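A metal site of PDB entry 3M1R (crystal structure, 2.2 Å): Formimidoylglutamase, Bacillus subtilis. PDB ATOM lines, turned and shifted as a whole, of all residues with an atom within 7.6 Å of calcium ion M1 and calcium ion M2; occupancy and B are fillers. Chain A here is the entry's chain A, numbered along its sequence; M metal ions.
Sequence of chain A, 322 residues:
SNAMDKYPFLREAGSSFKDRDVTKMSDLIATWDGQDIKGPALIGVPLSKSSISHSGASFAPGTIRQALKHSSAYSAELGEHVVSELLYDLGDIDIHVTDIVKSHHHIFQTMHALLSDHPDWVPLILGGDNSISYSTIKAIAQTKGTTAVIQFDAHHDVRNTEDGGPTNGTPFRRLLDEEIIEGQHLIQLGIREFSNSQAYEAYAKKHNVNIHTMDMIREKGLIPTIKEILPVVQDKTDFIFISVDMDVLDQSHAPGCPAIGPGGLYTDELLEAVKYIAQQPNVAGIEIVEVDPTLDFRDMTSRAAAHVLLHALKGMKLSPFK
Within 4 Å of calcium ion M2: Asn 130, Asp 153, Asp 157 and Asp 245. Along chain A the residues within 4 Å of calcium ion M2 span positions 130 to 245.
The side-chain amide nitrogen of Gln 151 sits close to the side-chain carboxylate of Asp 153. The backbone carbonyl oxygen (O) of Asp 153 is in hydrogen-bond range of the backbone NH (N) of Ile 191 (3.1 Å). The backbone carbonyl oxygen of Phe 152 sits at hydrogen-bond distance from the backbone NH of Asp 245 (2.9 Å). N of Asn 130 sits at hydrogen-bond distance from OE1 of Glu 290 (2.6 Å). OD1 of Asn 168 lies close to N of Asn 130, at 3.4 Å. The backbone carbonyl oxygen of Asn 130 is in hydrogen-bond range of the side-chain hydroxyl of Ser 133, at 2.9 Å. The backbone NH (N) of Phe 172 lies within hydrogen-bond range of the backbone carbonyl oxygen (O) of Asp 157 (3.2 Å).
Calcium ion M2 is bound by the side-chain carboxylate of Asp 153, the side-chain amide oxygen of Asn 130, the side-chain carboxylate of Asp 245, the side-chain carboxylate of Asp 157 and the side-chain amide nitrogen of Asn 130. Slightly farther from calcium ion M2 lies the side-chain carboxylate (OD1) of Asp 157 (3.0 Å).
Calcium ion M1 is bound by the side-chain carboxylate (OD2) of Asp 245 (2.3 Å), the side-chain carboxylate (OD2) of Asp 247 (2.3 Å), a ring nitrogen (ND1) of His 155 (2.4 Å), the side-chain carboxylate (OD1) of Asp 153 (2.4 Å) and the side-chain carboxylate (OD1) of Asp 247 (2.5 Å). Calcium ion M1 has five donor atoms within binding distance.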
ATOM      1  N   ASP A 129      18.082  17.605   3.188  1.00  0.00           N
ATOM      2  CA  ASP A 129      19.358  18.025   2.629  1.00  0.00           C
ATOM      3  C   ASP A 129      19.179  19.216   1.701  1.00  0.00           C
ATOM      4  O   ASP A 129      18.072  19.712   1.507  1.00  0.00           O
ATOM      5  CB  ASP A 129      20.069  16.860   1.931  1.00  0.00           C
ATOM      6  CG  ASP A 129      19.362  16.397   0.669  1.00  0.00           C
ATOM      7  OD1 ASP A 129      19.296  15.166   0.449  1.00  0.00           O
ATOM      8  OD2 ASP A 129      18.865  17.249  -0.097  1.00  0.00           O
ATOM      9  N   ASN A 130      20.291  19.666   1.135  1.00  0.00           N
ATOM     10  CA  ASN A 130      20.342  20.839   0.266  1.00  0.00           C
ATOM     11  C   ASN A 130      19.357  20.855  -0.889  1.00  0.00           C
ATOM     12  O   ASN A 130      18.866  21.918  -1.281  1.00  0.00           O
ATOM     13  CB  ASN A 130      21.718  20.912  -0.369  1.00  0.00           C
ATOM     14  CG  ASN A 130      22.518  22.039   0.156  1.00  0.00           C
ATOM     15  OD1 ASN A 130      23.726  21.910   0.286  1.00  0.00           O
ATOM     16  ND2 ASN A 130      21.868  23.169   0.459  1.00  0.00           N
ATOM     17  N   SER A 131      19.127  19.694  -1.493  1.00  0.00           N
ATOM     18  CA  SER A 131      18.410  19.648  -2.754  1.00  0.00           C
ATOM     19  C   SER A 131      16.974  20.144  -2.592  1.00  0.00           C
ATOM     20  O   SER A 131      16.327  20.486  -3.585  1.00  0.00           O
ATOM     21  CB  SER A 131      18.425  18.235  -3.369  1.00  0.00           C
ATOM     22  OG  SER A 131      17.723  17.332  -2.543  1.00  0.00           O
ATOM     23  N   SER A 133      16.079  22.915  -1.601  1.00  0.00           N
ATOM     24  CA  SER A 133      16.043  24.366  -1.879  1.00  0.00           C
ATOM     25  C   SER A 133      15.453  24.708  -3.256  1.00  0.00           C
ATOM     26  O   SER A 133      14.799  25.745  -3.432  1.00  0.00           O
ATOM     27  CB  SER A 133      17.448  24.958  -1.751  1.00  0.00           C
ATOM     28  OG  SER A 133      18.003  24.607  -0.500  1.00  0.00           O
ATOM     29  N   GLN A 151      21.715  32.947   0.651  1.00  0.00           N
ATOM     30  CA  GLN A 151      22.164  31.617   1.010  1.00  0.00           C
ATOM     31  C   GLN A 151      23.472  31.669   1.786  1.00  0.00           C
ATOM     32  O   GLN A 151      24.490  32.170   1.284  1.00  0.00           O
ATOM     33  CB  GLN A 151      22.235  30.685  -0.213  1.00  0.00           C
ATOM     34  CG  GLN A 151      23.383  30.951  -1.164  1.00  0.00           C
ATOM     35  CD  GLN A 151      23.620  29.797  -2.145  1.00  0.00           C
ATOM     36  OE1 GLN A 151      23.539  29.973  -3.349  1.00  0.00           O
ATOM     37  NE2 GLN A 151      23.931  28.609  -1.610  1.00  0.00           N
ATOM     38  N   PHE A 152      23.405  31.197   3.024  1.00  0.00           N
ATOM     39  CA  PHE A 152      24.598  30.958   3.817  1.00  0.00           C
ATOM     40  C   PHE A 152      25.116  29.584   3.429  1.00  0.00           C
ATOM     41  O   PHE A 152      24.356  28.595   3.469  1.00  0.00           O
ATOM     42  CB  PHE A 152      24.287  30.984   5.309  1.00  0.00           C
ATOM     43  CG  PHE A 152      23.845  32.323   5.828  1.00  0.00           C
ATOM     44  CD1 PHE A 152      24.776  33.216   6.340  1.00  0.00           C
ATOM     45  CD2 PHE A 152      22.529  32.686   5.823  1.00  0.00           C
ATOM     46  CE1 PHE A 152      24.387  34.457   6.831  1.00  0.00           C
ATOM     47  CE2 PHE A 152      22.120  33.936   6.310  1.00  0.00           C
ATOM     48  CZ  PHE A 152      23.053  34.807   6.805  1.00  0.00           C
ATOM     49  N   ASP A 153      26.395  29.498   3.090  1.00  0.00           N
ATOM     50  CA  ASP A 153      26.921  28.276   2.515  1.00  0.00           C
ATOM     51  C   ASP A 153      28.409  28.395   2.264  1.00  0.00           C
ATOM     52  O   ASP A 153      28.904  29.438   1.865  1.00  0.00           O
ATOM     53  CB  ASP A 153      26.213  28.030   1.192  1.00  0.00           C
ATOM     54  CG  ASP A 153      26.334  26.613   0.751  1.00  0.00           C
ATOM     55  OD1 ASP A 153      27.327  25.965   1.123  1.00  0.00           O
ATOM     56  OD2 ASP A 153      25.444  26.156   0.022  1.00  0.00           O
ATOM     57  N   ALA A 154      29.131  27.297   2.520  1.00  0.00           N
ATOM     58  CA  ALA A 154      30.536  27.200   2.125  1.00  0.00           C
ATOM     59  C   ALA A 154      30.648  26.911   0.617  1.00  0.00           C
ATOM     60  O   ALA A 154      31.654  27.244  -0.005  1.00  0.00           O
ATOM     61  CB  ALA A 154      31.248  26.098   2.946  1.00  0.00           C
ATOM     62  N   HIS A 155      29.613  26.303   0.049  1.00  0.00           N
ATOM     63  CA  HIS A 155      29.622  25.858  -1.361  1.00  0.00           C
ATOM     64  C   HIS A 155      28.659  26.645  -2.253  1.00  0.00           C
ATOM     65  O   HIS A 155      27.609  27.141  -1.797  1.00  0.00           O
ATOM     66  CB  HIS A 155      29.273  24.364  -1.437  1.00  0.00           C
ATOM     67  CG  HIS A 155      29.995  23.548  -0.407  1.00  0.00           C
ATOM     68  ND1 HIS A 155      29.399  23.175   0.774  1.00  0.00           N
ATOM     69  CD2 HIS A 155      31.253  23.083  -0.362  1.00  0.00           C
ATOM     70  CE1 HIS A 155      30.263  22.478   1.506  1.00  0.00           C
ATOM     71  NE2 HIS A 155      31.398  22.403   0.835  1.00  0.00           N
ATOM     72  N   HIS A 156      29.019  26.761  -3.524  1.00  0.00           N
ATOM     73  CA  HIS A 156      28.193  27.514  -4.441  1.00  0.00           C
ATOM     74  C   HIS A 156      26.886  26.794  -4.647  1.00  0.00           C
ATOM     75  O   HIS A 156      25.865  27.415  -4.862  1.00  0.00           O
ATOM     76  CB  HIS A 156      28.912  27.688  -5.781  1.00  0.00           C
ATOM     77  CG  HIS A 156      30.038  28.670  -5.740  1.00  0.00           C
ATOM     78  ND1 HIS A 156      29.834  30.014  -5.545  1.00  0.00           N
ATOM     79  CD2 HIS A 156      31.375  28.498  -5.913  1.00  0.00           C
ATOM     80  CE1 HIS A 156      31.008  30.642  -5.575  1.00  0.00           C
ATOM     81  NE2 HIS A 156      31.956  29.745  -5.797  1.00  0.00           N
ATOM     82  N   ASP A 157      26.922  25.462  -4.558  1.00  0.00           N
ATOM     83  CA  ASP A 157      25.775  24.608  -4.879  1.00  0.00           C
ATOM     84  C   ASP A 157      25.238  24.800  -6.296  1.00  0.00           C
ATOM     85  O   ASP A 157      24.024  24.912  -6.513  1.00  0.00           O
ATOM     86  CB  ASP A 157      24.639  24.798  -3.869  1.00  0.00           C
ATOM     87  CG  ASP A 157      24.834  23.933  -2.615  1.00  0.00           C
ATOM     88  OD1 ASP A 157      25.986  23.790  -2.167  1.00  0.00           O
ATOM     89  OD2 ASP A 157      23.827  23.399  -2.103  1.00  0.00           O
ATOM     90  N   ASN A 168      22.766  16.463  -4.832  1.00  0.00           N
ATOM     91  CA  ASN A 168      22.768  17.255  -3.601  1.00  0.00           C
ATOM     92  C   ASN A 168      23.164  18.710  -3.819  1.00  0.00           C
ATOM     93  O   ASN A 168      22.535  19.608  -3.274  1.00  0.00           O
ATOM     94  CB  ASN A 168      23.602  16.622  -2.475  1.00  0.00           C
ATOM     95  CG  ASN A 168      23.222  17.173  -1.116  1.00  0.00           C
ATOM     96  OD1 ASN A 168      22.121  17.736  -0.977  1.00  0.00           O
ATOM     97  ND2 ASN A 168      24.101  17.049  -0.137  1.00  0.00           N
ATOM     98  N   GLY A 169      24.206  18.928  -4.605  1.00  0.00           N
ATOM     99  CA  GLY A 169      24.745  20.263  -4.798  1.00  0.00           C
ATOM    100  C   GLY A 169      24.277  20.934  -6.075  1.00  0.00           C
ATOM    101  O   GLY A 169      24.991  21.780  -6.615  1.00  0.00           O
ATOM    102  N   PRO A 171      20.893  22.463  -6.456  1.00  0.00           N
ATOM    103  CA  PRO A 171      19.680  23.309  -6.395  1.00  0.00           C
ATOM    104  C   PRO A 171      19.800  24.663  -7.084  1.00  0.00           C
ATOM    105  O   PRO A 171      18.886  25.051  -7.802  1.00  0.00           O
ATOM    106  CB  PRO A 171      19.440  23.497  -4.904  1.00  0.00           C
ATOM    107  CG  PRO A 171      20.763  23.126  -4.230  1.00  0.00           C
ATOM    108  CD  PRO A 171      21.332  22.044  -5.119  1.00  0.00           C
ATOM    109  N   PHE A 172      20.904  25.373  -6.871  1.00  0.00           N
ATOM    110  CA  PHE A 172      21.006  26.707  -7.460  1.00  0.00           C
ATOM    111  C   PHE A 172      21.345  26.746  -8.942  1.00  0.00           C
ATOM    112  O   PHE A 172      21.196  27.788  -9.586  1.00  0.00           O
ATOM    113  CB  PHE A 172      21.891  27.619  -6.614  1.00  0.00           C
ATOM    114  CG  PHE A 172      21.334  27.883  -5.260  1.00  0.00           C
ATOM    115  CD1 PHE A 172      21.721  27.117  -4.176  1.00  0.00           C
ATOM    116  CD2 PHE A 172      20.383  28.866  -5.073  1.00  0.00           C
ATOM    117  CE1 PHE A 172      21.187  27.353  -2.927  1.00  0.00           C
ATOM    118  CE2 PHE A 172      19.841  29.110  -3.837  1.00  0.00           C
ATOM    119  CZ  PHE A 172      20.245  28.347  -2.755  1.00  0.00           C
ATOM    120  N   ILE A 191      31.116  31.540   1.314  1.00  0.00           N
ATOM    121  CA  ILE A 191      31.839  30.706   0.372  1.00  0.00           C
ATOM    122  C   ILE A 191      33.313  30.539   0.777  1.00  0.00           C
ATOM    123  O   ILE A 191      34.031  31.516   0.955  1.00  0.00           O
ATOM    124  CB  ILE A 191      31.753  31.253  -1.070  1.00  0.00           C
ATOM    125  CG1 ILE A 191      30.281  31.293  -1.529  1.00  0.00           C
ATOM    126  CG2 ILE A 191      32.620  30.400  -2.008  1.00  0.00           C
ATOM    127  CD1 ILE A 191      29.622  29.931  -1.711  1.00  0.00           C
ATOM    128  N   SER A 195      36.596  24.799  -0.770  1.00  0.00           N
ATOM    129  CA  SER A 195      35.321  24.103  -0.728  1.00  0.00           C
ATOM    130  C   SER A 195      34.642  24.033  -2.109  1.00  0.00           C
ATOM    131  O   SER A 195      33.595  23.419  -2.256  1.00  0.00           O
ATOM    132  CB  SER A 195      34.370  24.749   0.309  1.00  0.00           C
ATOM    133  OG  SER A 195      34.636  24.285   1.618  1.00  0.00           O
ATOM    134  N   ASN A 196      35.261  24.645  -3.123  1.00  0.00           N
ATOM    135  CA  ASN A 196      34.619  24.776  -4.441  1.00  0.00           C
ATOM    136  C   ASN A 196      35.479  24.451  -5.654  1.00  0.00           C
ATOM    137  O   ASN A 196      36.687  24.269  -5.536  1.00  0.00           O
ATOM    138  CB  ASN A 196      34.060  26.189  -4.609  1.00  0.00           C
ATOM    139  CG  ASN A 196      32.976  26.487  -3.625  1.00  0.00           C
ATOM    140  OD1 ASN A 196      31.847  26.034  -3.784  1.00  0.00           O
ATOM    141  ND2 ASN A 196      33.326  27.191  -2.553  1.00  0.00           N
ATOM    142  N   SER A 243      18.140  31.083   2.975  1.00  0.00           N
ATOM    143  CA  SER A 243      18.545  29.664   2.931  1.00  0.00           C
ATOM    144  C   SER A 243      19.778  29.447   3.807  1.00  0.00           C
ATOM    145  O   SER A 243      20.873  29.954   3.511  1.00  0.00           O
ATOM    146  CB  SER A 243      18.827  29.184   1.510  1.00  0.00           C
ATOM    147  OG  SER A 243      18.857  27.762   1.457  1.00  0.00           O
ATOM    148  N   VAL A 244      19.603  28.723   4.899  1.00  0.00           N
ATOM    149  CA  VAL A 244      20.733  28.504   5.793  1.00  0.00           C
ATOM    150  C   VAL A 244      21.283  27.079   5.612  1.00  0.00           C
ATOM    151  O   VAL A 244      20.685  26.118   6.093  1.00  0.00           O
ATOM    152  CB  VAL A 244      20.345  28.725   7.260  1.00  0.00           C
ATOM    153  CG1 VAL A 244      21.485  28.247   8.188  1.00  0.00           C
ATOM    154  CG2 VAL A 244      20.014  30.186   7.522  1.00  0.00           C
ATOM    155  N   ASP A 245      22.400  26.951   4.916  1.00  0.00           N
ATOM    156  CA  ASP A 245      23.094  25.657   4.894  1.00  0.00           C
ATOM    157  C   ASP A 245      24.062  25.620   6.079  1.00  0.00           C
ATOM    158  O   ASP A 245      25.030  26.376   6.103  1.00  0.00           O
ATOM    159  CB  ASP A 245      23.867  25.433   3.592  1.00  0.00           C
ATOM    160  CG  ASP A 245      24.705  24.153   3.627  1.00  0.00           C
ATOM    161  OD1 ASP A 245      24.937  23.574   4.716  1.00  0.00           O
ATOM    162  OD2 ASP A 245      25.123  23.705   2.566  1.00  0.00           O
ATOM    163  N   MET A 246      23.790  24.748   7.039  1.00  0.00           N
ATOM    164  CA  MET A 246      24.527  24.731   8.293  1.00  0.00           C
ATOM    165  C   MET A 246      26.024  24.459   8.115  1.00  0.00           C
ATOM    166  O   MET A 246      26.814  24.749   9.019  1.00  0.00           O
ATOM    167  CB  MET A 246      23.914  23.728   9.294  1.00  0.00           C
ATOM    168  CG  MET A 246      22.501  24.138   9.810  1.00  0.00           C
ATOM    169  SD  MET A 246      22.482  25.875  10.739  1.00  0.00           S
ATOM    170  CE  MET A 246      23.106  25.311  12.515  1.00  0.00           C
ATOM    171  N   ASP A 247      26.419  23.909   6.976  1.00  0.00           N
ATOM    172  CA  ASP A 247      27.834  23.651   6.759  1.00  0.00           C
ATOM    173  C   ASP A 247      28.591  24.935   6.452  1.00  0.00           C
ATOM    174  O   ASP A 247      29.797  24.911   6.227  1.00  0.00           O
ATOM    175  CB  ASP A 247      28.066  22.551   5.690  1.00  0.00           C
ATOM    176  CG  ASP A 247      27.761  23.024   4.293  1.00  0.00           C
ATOM    177  OD1 ASP A 247      27.919  24.234   3.980  1.00  0.00           O
ATOM    178  OD2 ASP A 247      27.381  22.162   3.475  1.00  0.00           O
ATOM    179  N   VAL A 248      27.889  26.071   6.461  1.00  0.00           N
ATOM    180  CA  VAL A 248      28.572  27.348   6.411  1.00  0.00           C
ATOM    181  C   VAL A 248      29.349  27.508   7.726  1.00  0.00           C
ATOM    182  O   VAL A 248      30.320  28.243   7.805  1.00  0.00           O
ATOM    183  CB  VAL A 248      27.594  28.536   6.248  1.00  0.00           C
ATOM    184  CG1 VAL A 248      26.900  28.843   7.577  1.00  0.00           C
ATOM    185  CG2 VAL A 248      28.323  29.781   5.712  1.00  0.00           C
ATOM    186  N   ALA A 259      29.431  17.902   5.143  1.00  0.00           N
ATOM    187  CA  ALA A 259      30.634  18.620   4.697  1.00  0.00           C
ATOM    188  C   ALA A 259      31.231  19.557   5.748  1.00  0.00           C
ATOM    189  O   ALA A 259      30.934  20.736   5.774  1.00  0.00           O
ATOM    190  CB  ALA A 259      30.364  19.410   3.395  1.00  0.00           C
ATOM    191  N   VAL A 289      19.215  23.588   6.063  1.00  0.00           N
ATOM    192  CA  VAL A 289      19.577  22.332   5.445  1.00  0.00           C
ATOM    193  C   VAL A 289      20.901  21.768   5.975  1.00  0.00           C
ATOM    194  O   VAL A 289      21.634  22.455   6.683  1.00  0.00           O
ATOM    195  CB  VAL A 289      19.668  22.468   3.912  1.00  0.00           C
ATOM    196  CG1 VAL A 289      18.336  22.946   3.355  1.00  0.00           C
ATOM    197  CG2 VAL A 289      20.786  23.436   3.546  1.00  0.00           C
ATOM    198  N   GLU A 290      21.167  20.509   5.631  1.00  0.00           N
ATOM    199  CA  GLU A 290      22.441  19.867   5.888  1.00  0.00           C
ATOM    200  C   GLU A 290      22.775  19.668   7.369  1.00  0.00           C
ATOM    201  O   GLU A 290      23.949  19.602   7.737  1.00  0.00           O
ATOM    202  CB  GLU A 290      23.574  20.601   5.158  1.00  0.00           C
ATOM    203  CG  GLU A 290      23.397  20.599   3.621  1.00  0.00           C
ATOM    204  CD  GLU A 290      23.427  19.181   3.024  1.00  0.00           C
ATOM    205  OE1 GLU A 290      22.611  18.879   2.137  1.00  0.00           O
ATOM    206  OE2 GLU A 290      24.258  18.367   3.479  1.00  0.00           O
HETATM  207 CA    CA M   1      27.236  23.632   1.661  1.00  0.00          CA
HETATM  208 CA    CA M   2      24.396  24.147   0.341  1.00  0.00          CA
